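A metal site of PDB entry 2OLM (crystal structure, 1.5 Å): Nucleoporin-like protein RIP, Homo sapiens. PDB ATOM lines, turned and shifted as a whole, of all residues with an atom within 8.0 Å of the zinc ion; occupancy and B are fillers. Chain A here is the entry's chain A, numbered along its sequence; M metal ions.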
ATOM      1  N   LYS A  27     -33.188 -17.902  -9.617  1.00  0.00           N
ATOM      2  CA  LYS A  27     -32.134 -17.952  -8.627  1.00  0.00           C
ATOM      3  C   LYS A  27     -31.232 -16.745  -8.838  1.00  0.00           C
ATOM      4  O   LYS A  27     -31.005 -16.321  -9.980  1.00  0.00           O
ATOM      5  CB  LYS A  27     -31.305 -19.231  -8.776  1.00  0.00           C
ATOM      6  CG  LYS A  27     -32.087 -20.493  -8.467  1.00  0.00           C
ATOM      7  CD  LYS A  27     -32.421 -20.581  -7.017  1.00  0.00           C
ATOM      8  N   CYS A  28     -30.760 -16.205  -7.724  1.00  0.00           N
ATOM      9  CA  CYS A  28     -29.785 -15.066  -7.717  1.00  0.00           C
ATOM     10  C   CYS A  28     -28.645 -15.384  -8.673  1.00  0.00           C
ATOM     11  O   CYS A  28     -28.037 -16.436  -8.574  1.00  0.00           O
ATOM     12  CB  CYS A  28     -29.231 -14.855  -6.327  1.00  0.00           C
ATOM     13  SG  CYS A  28     -28.007 -13.594  -6.295  1.00  0.00           S
ATOM     14  N   PHE A  29     -28.304 -14.451  -9.574  1.00  0.00           N
ATOM     15  CA  PHE A  29     -27.208 -14.638 -10.533  1.00  0.00           C
ATOM     16  C   PHE A  29     -25.857 -14.785  -9.845  1.00  0.00           C
ATOM     17  O   PHE A  29     -24.960 -15.397 -10.409  1.00  0.00           O
ATOM     18  CB  PHE A  29     -27.152 -13.484 -11.488  1.00  0.00           C
ATOM     19  CG  PHE A  29     -26.117 -13.643 -12.522  1.00  0.00           C
ATOM     20  CD1 PHE A  29     -26.121 -14.733 -13.355  1.00  0.00           C
ATOM     21  CD2 PHE A  29     -25.110 -12.692 -12.672  1.00  0.00           C
ATOM     22  CE1 PHE A  29     -25.100 -14.933 -14.279  1.00  0.00           C
ATOM     23  CE2 PHE A  29     -24.113 -12.865 -13.625  1.00  0.00           C
ATOM     24  CZ  PHE A  29     -24.115 -13.976 -14.420  1.00  0.00           C
ATOM     25  N   ASP A  30     -25.661 -14.190  -8.694  1.00  0.00           N
ATOM     26  CA  ASP A  30     -24.371 -14.183  -8.060  1.00  0.00           C
ATOM     27  C   ASP A  30     -24.114 -15.300  -7.061  1.00  0.00           C
ATOM     28  O   ASP A  30     -23.009 -15.853  -7.026  1.00  0.00           O
ATOM     29  CB  ASP A  30     -24.050 -12.787  -7.446  1.00  0.00           C
ATOM     30  CG  ASP A  30     -23.905 -11.740  -8.531  1.00  0.00           C
ATOM     31  OD1 ASP A  30     -23.115 -12.007  -9.503  1.00  0.00           O
ATOM     32  OD2 ASP A  30     -24.577 -10.697  -8.445  1.00  0.00           O
ATOM     33  N   CYS A  31     -25.103 -15.621  -6.239  1.00  0.00           N
ATOM     34  CA  CYS A  31     -24.938 -16.742  -5.291  1.00  0.00           C
ATOM     35  C   CYS A  31     -25.662 -18.028  -5.634  1.00  0.00           C
ATOM     36  O   CYS A  31     -25.311 -19.080  -5.060  1.00  0.00           O
ATOM     37  CB  CYS A  31     -25.304 -16.308  -3.869  1.00  0.00           C
ATOM     38  SG  CYS A  31     -27.071 -16.070  -3.557  1.00  0.00           S
ATOM     39  N   ASP A  32     -26.675 -17.970  -6.504  1.00  0.00           N
ATOM     40  CA  ASP A  32     -27.465 -19.150  -6.875  1.00  0.00           C
ATOM     41  C   ASP A  32     -28.131 -19.820  -5.683  1.00  0.00           C
ATOM     42  O   ASP A  32     -28.499 -20.997  -5.781  1.00  0.00           O
ATOM     43  CB  ASP A  32     -26.568 -20.167  -7.633  1.00  0.00           C
ATOM     44  CG  ASP A  32     -27.369 -21.182  -8.416  1.00  0.00           C
ATOM     45  OD1 ASP A  32     -28.266 -20.778  -9.138  1.00  0.00           O
ATOM     46  OD2 ASP A  32     -27.087 -22.407  -8.285  1.00  0.00           O
ATOM     47  N   GLN A  33     -28.298 -19.091  -4.577  1.00  0.00           N
ATOM     48  CA  GLN A  33     -28.739 -19.741  -3.311  1.00  0.00           C
ATOM     49  C   GLN A  33     -30.156 -19.434  -2.974  1.00  0.00           C
ATOM     50  O   GLN A  33     -30.749 -20.108  -2.138  1.00  0.00           O
ATOM     51  CB  GLN A  33     -27.898 -19.285  -2.119  1.00  0.00           C
ATOM     52  CG  GLN A  33     -26.470 -19.787  -2.078  1.00  0.00           C
ATOM     53  CD  GLN A  33     -25.816 -19.594  -0.723  1.00  0.00           C
ATOM     54  OE1 GLN A  33     -25.918 -18.529  -0.107  1.00  0.00           O
ATOM     55  NE2 GLN A  33     -25.099 -20.617  -0.266  1.00  0.00           N
ATOM     56  N   ARG A  34     -30.712 -18.389  -3.569  1.00  0.00           N
ATOM     57  CA  ARG A  34     -32.091 -18.053  -3.281  1.00  0.00           C
ATOM     58  C   ARG A  34     -32.714 -17.223  -4.373  1.00  0.00           C
ATOM     59  O   ARG A  34     -32.040 -16.858  -5.338  1.00  0.00           O
ATOM     60  CB  ARG A  34     -32.170 -17.300  -1.986  1.00  0.00           C
ATOM     61  CG  ARG A  34     -31.421 -16.017  -2.036  1.00  0.00           C
ATOM     62  CD  ARG A  34     -31.414 -15.391  -0.678  1.00  0.00           C
ATOM     63  NE  ARG A  34     -30.686 -16.209   0.291  1.00  0.00           N
ATOM     64  CZ  ARG A  34     -29.370 -16.138   0.513  1.00  0.00           C
ATOM     65  NH1 ARG A  34     -28.584 -15.301  -0.158  1.00  0.00           N
ATOM     66  NH2 ARG A  34     -28.821 -16.938   1.439  1.00  0.00           N
ATOM     67  N   GLY A  35     -34.006 -16.957  -4.220  1.00  0.00           N
ATOM     68  CA  GLY A  35     -34.737 -16.171  -5.177  1.00  0.00           C
ATOM     69  C   GLY A  35     -34.322 -14.715  -5.207  1.00  0.00           C
ATOM     70  O   GLY A  35     -33.941 -14.140  -4.167  1.00  0.00           O
ATOM     71  N   PRO A  36     -34.330 -14.136  -6.395  1.00  0.00           N
ATOM     72  CA  PRO A  36     -34.005 -12.723  -6.501  1.00  0.00           C
ATOM     73  C   PRO A  36     -35.095 -11.796  -5.996  1.00  0.00           C
ATOM     74  O   PRO A  36     -36.285 -12.072  -6.127  1.00  0.00           O
ATOM     75  CB  PRO A  36     -33.751 -12.512  -7.990  1.00  0.00           C
ATOM     76  CG  PRO A  36     -34.401 -13.598  -8.667  1.00  0.00           C
ATOM     77  CD  PRO A  36     -34.569 -14.745  -7.710  1.00  0.00           C
ATOM     78  N   THR A  37     -34.625 -10.676  -5.459  1.00  0.00           N
ATOM     79  CA  THR A  37     -35.441  -9.590  -4.950  1.00  0.00           C
ATOM     80  C   THR A  37     -35.125  -8.235  -5.630  1.00  0.00           C
ATOM     81  O   THR A  37     -35.867  -7.273  -5.485  1.00  0.00           O
ATOM     82  CB  THR A  37     -35.177  -9.422  -3.453  1.00  0.00           C
ATOM     83  OG1 THR A  37     -33.770  -9.444  -3.197  1.00  0.00           O
ATOM     84  CG2 THR A  37     -35.812 -10.596  -2.667  1.00  0.00           C
ATOM     85  N   PHE A  46     -30.707 -10.666 -12.203  1.00  0.00           N
ATOM     86  CA  PHE A  46     -31.663 -10.750 -11.092  1.00  0.00           C
ATOM     87  C   PHE A  46     -30.948 -11.330  -9.919  1.00  0.00           C
ATOM     88  O   PHE A  46     -30.380 -12.436 -10.008  1.00  0.00           O
ATOM     89  CB  PHE A  46     -32.882 -11.631 -11.497  1.00  0.00           C
ATOM     90  CG  PHE A  46     -33.706 -11.057 -12.587  1.00  0.00           C
ATOM     91  CD1 PHE A  46     -34.869 -10.385 -12.303  1.00  0.00           C
ATOM     92  CD2 PHE A  46     -33.308 -11.137 -13.901  1.00  0.00           C
ATOM     93  CE1 PHE A  46     -35.624  -9.804 -13.316  1.00  0.00           C
ATOM     94  CE2 PHE A  46     -34.054 -10.566 -14.897  1.00  0.00           C
ATOM     95  CZ  PHE A  46     -35.227  -9.910 -14.606  1.00  0.00           C
ATOM     96  N   VAL A  47     -30.914 -10.596  -8.775  1.00  0.00           N
ATOM     97  CA  VAL A  47     -30.055 -10.921  -7.631  1.00  0.00           C
ATOM     98  C   VAL A  47     -30.846 -10.829  -6.310  1.00  0.00           C
ATOM     99  O   VAL A  47     -31.874 -10.172  -6.245  1.00  0.00           O
ATOM    100  CB  VAL A  47     -28.809  -9.994  -7.541  1.00  0.00           C
ATOM    101  CG1 VAL A  47     -27.894 -10.291  -8.723  1.00  0.00           C
ATOM    102  CG2 VAL A  47     -29.218  -8.498  -7.603  1.00  0.00           C
ATOM    103  N   CYS A  48     -30.309 -11.440  -5.277  1.00  0.00           N
ATOM    104  CA  CYS A  48     -30.937 -11.460  -3.944  1.00  0.00           C
ATOM    105  C   CYS A  48     -30.496 -10.219  -3.148  1.00  0.00           C
ATOM    106  O   CYS A  48     -29.628  -9.435  -3.608  1.00  0.00           O
ATOM    107  CB  CYS A  48     -30.545 -12.756  -3.209  1.00  0.00           C
ATOM    108  SG  CYS A  48     -28.883 -12.845  -2.546  1.00  0.00           S
ATOM    109  N   THR A  49     -31.073  -9.994  -1.954  1.00  0.00           N
ATOM    110  CA  THR A  49     -30.728  -8.842  -1.177  1.00  0.00           C
ATOM    111  C   THR A  49     -29.330  -8.817  -0.654  1.00  0.00           C
ATOM    112  O   THR A  49     -28.668  -7.778  -0.658  1.00  0.00           O
ATOM    113  CB  THR A  49     -31.771  -8.701  -0.035  1.00  0.00           C
ATOM    114  OG1 THR A  49     -33.083  -8.645  -0.619  1.00  0.00           O
ATOM    115  CG2 THR A  49     -31.436  -7.504   0.820  1.00  0.00           C
ATOM    116  N   SER A  50     -28.819  -9.971  -0.209  1.00  0.00           N
ATOM    117  CA  SER A  50     -27.505 -10.040   0.326  1.00  0.00           C
ATOM    118  C   SER A  50     -26.450  -9.727  -0.742  1.00  0.00           C
ATOM    119  O   SER A  50     -25.535  -8.960  -0.523  1.00  0.00           O
ATOM    120  CB  SER A  50     -27.259 -11.403   0.967  1.00  0.00           C
ATOM    121  OG  SER A  50     -25.995 -11.429   1.550  1.00  0.00           O
ATOM    122  N   CYS A  51     -26.627 -10.332  -1.916  1.00  0.00           N
ATOM    123  CA  CYS A  51     -25.689 -10.033  -2.982  1.00  0.00           C
ATOM    124  C   CYS A  51     -25.817  -8.597  -3.426  1.00  0.00           C
ATOM    125  O   CYS A  51     -24.776  -7.992  -3.736  1.00  0.00           O
ATOM    126  CB  CYS A  51     -25.920 -10.952  -4.158  1.00  0.00           C
ATOM    127  SG  CYS A  51     -25.342 -12.680  -3.848  1.00  0.00           S
ATOM    128  N   SER A  52     -27.038  -8.041  -3.425  1.00  0.00           N
ATOM    129  CA  SER A  52     -27.206  -6.620  -3.742  1.00  0.00           C
ATOM    130  C   SER A  52     -26.387  -5.750  -2.785  1.00  0.00           C
ATOM    131  O   SER A  52     -25.730  -4.778  -3.193  1.00  0.00           O
ATOM    132  CB  SER A  52     -28.648  -6.228  -3.685  1.00  0.00           C
ATOM    133  OG  SER A  52     -29.424  -6.871  -4.673  1.00  0.00           O
ATOM    134  N   LEU A  55     -22.780  -6.031  -3.963  1.00  0.00           N
ATOM    135  CA  LEU A  55     -22.619  -5.323  -5.245  1.00  0.00           C
ATOM    136  C   LEU A  55     -22.480  -3.835  -5.023  1.00  0.00           C
ATOM    137  O   LEU A  55     -21.785  -3.141  -5.816  1.00  0.00           O
ATOM    138  CB  LEU A  55     -23.820  -5.607  -6.113  1.00  0.00           C
ATOM    139  CG  LEU A  55     -23.857  -7.020  -6.781  1.00  0.00           C
ATOM    140  CD1 LEU A  55     -25.263  -7.364  -7.283  1.00  0.00           C
ATOM    141  CD2 LEU A  55     -22.804  -7.145  -7.931  1.00  0.00           C
ATOM    142  N   PHE A 106     -20.668 -17.593   1.038  1.00  0.00           N
ATOM    143  CA  PHE A 106     -21.538 -16.443   0.898  1.00  0.00           C
ATOM    144  C   PHE A 106     -22.017 -15.849   2.235  1.00  0.00           C
ATOM    145  O   PHE A 106     -22.616 -14.773   2.249  1.00  0.00           O
ATOM    146  CB  PHE A 106     -22.683 -16.764  -0.051  1.00  0.00           C
ATOM    147  CG  PHE A 106     -22.256 -16.782  -1.517  1.00  0.00           C
ATOM    148  CD1 PHE A 106     -22.126 -15.584  -2.234  1.00  0.00           C
ATOM    149  CD2 PHE A 106     -21.965 -17.987  -2.169  1.00  0.00           C
ATOM    150  CE1 PHE A 106     -21.710 -15.595  -3.570  1.00  0.00           C
ATOM    151  CE2 PHE A 106     -21.553 -17.995  -3.529  1.00  0.00           C
ATOM    152  CZ  PHE A 106     -21.416 -16.781  -4.207  1.00  0.00           C
ATOM    153  N   VAL A 112     -17.269 -12.484  -0.324  1.00  0.00           N
ATOM    154  CA  VAL A 112     -18.228 -12.223  -1.418  1.00  0.00           C
ATOM    155  C   VAL A 112     -17.724 -11.020  -2.236  1.00  0.00           C
ATOM    156  O   VAL A 112     -17.680 -11.073  -3.465  1.00  0.00           O
ATOM    157  CB  VAL A 112     -19.670 -12.037  -0.916  1.00  0.00           C
ATOM    158  CG1 VAL A 112     -20.591 -11.635  -2.039  1.00  0.00           C
ATOM    159  CG2 VAL A 112     -20.192 -13.349  -0.261  1.00  0.00           C
ATOM    160  N   LEU A 116     -16.958 -11.069  -6.250  1.00  0.00           N
ATOM    161  CA  LEU A 116     -17.615 -10.174  -7.176  1.00  0.00           C
ATOM    162  C   LEU A 116     -16.583  -9.310  -7.941  1.00  0.00           C
ATOM    163  O   LEU A 116     -16.743  -9.031  -9.127  1.00  0.00           O
ATOM    164  CB  LEU A 116     -18.642  -9.304  -6.470  1.00  0.00           C
ATOM    165  CG  LEU A 116     -19.785 -10.019  -5.809  1.00  0.00           C
ATOM    166  CD1 LEU A 116     -20.607  -8.985  -4.996  1.00  0.00           C
ATOM    167  CD2 LEU A 116     -20.650 -10.708  -6.772  1.00  0.00           C
HETATM  168 ZN    ZN M   1     -27.388 -13.838  -3.989  1.00  0.00          ZN
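The side-chain hydroxyl (OG) of Ser 52 is in hydrogen-bond range of the backbone carbonyl oxygen (O) of Cys 48 (2.8 Å).
N of Asp 30 sits close to SG of Cys 28 (3.4 Å).
The side-chain sulfur (SG) of Cys 48 sits close to the backbone NH (N) of Ser 50, 3.7 Å away.
The guanidinium group (NH1) of Arg 34 lies close to the side-chain sulfur (SG) of Cys 48.
N of Cys 28 sits at hydrogen-bond distance from O of Arg 34 (2.8 Å).
The guanidinium group (NH1) of Arg 34 lies close to the side-chain sulfur (SG) of Cys 31, at 3.8 Å.
The side-chain sulfur of Cys 31 sits close to the backbone NH of Gln 33.
The zinc ion is bound by SG of Cys 31 (2.3 Å), SG of Cys 48 (2.3 Å), SG of Cys 51 (2.4 Å) and SG of Cys 28 (2.4 Å).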
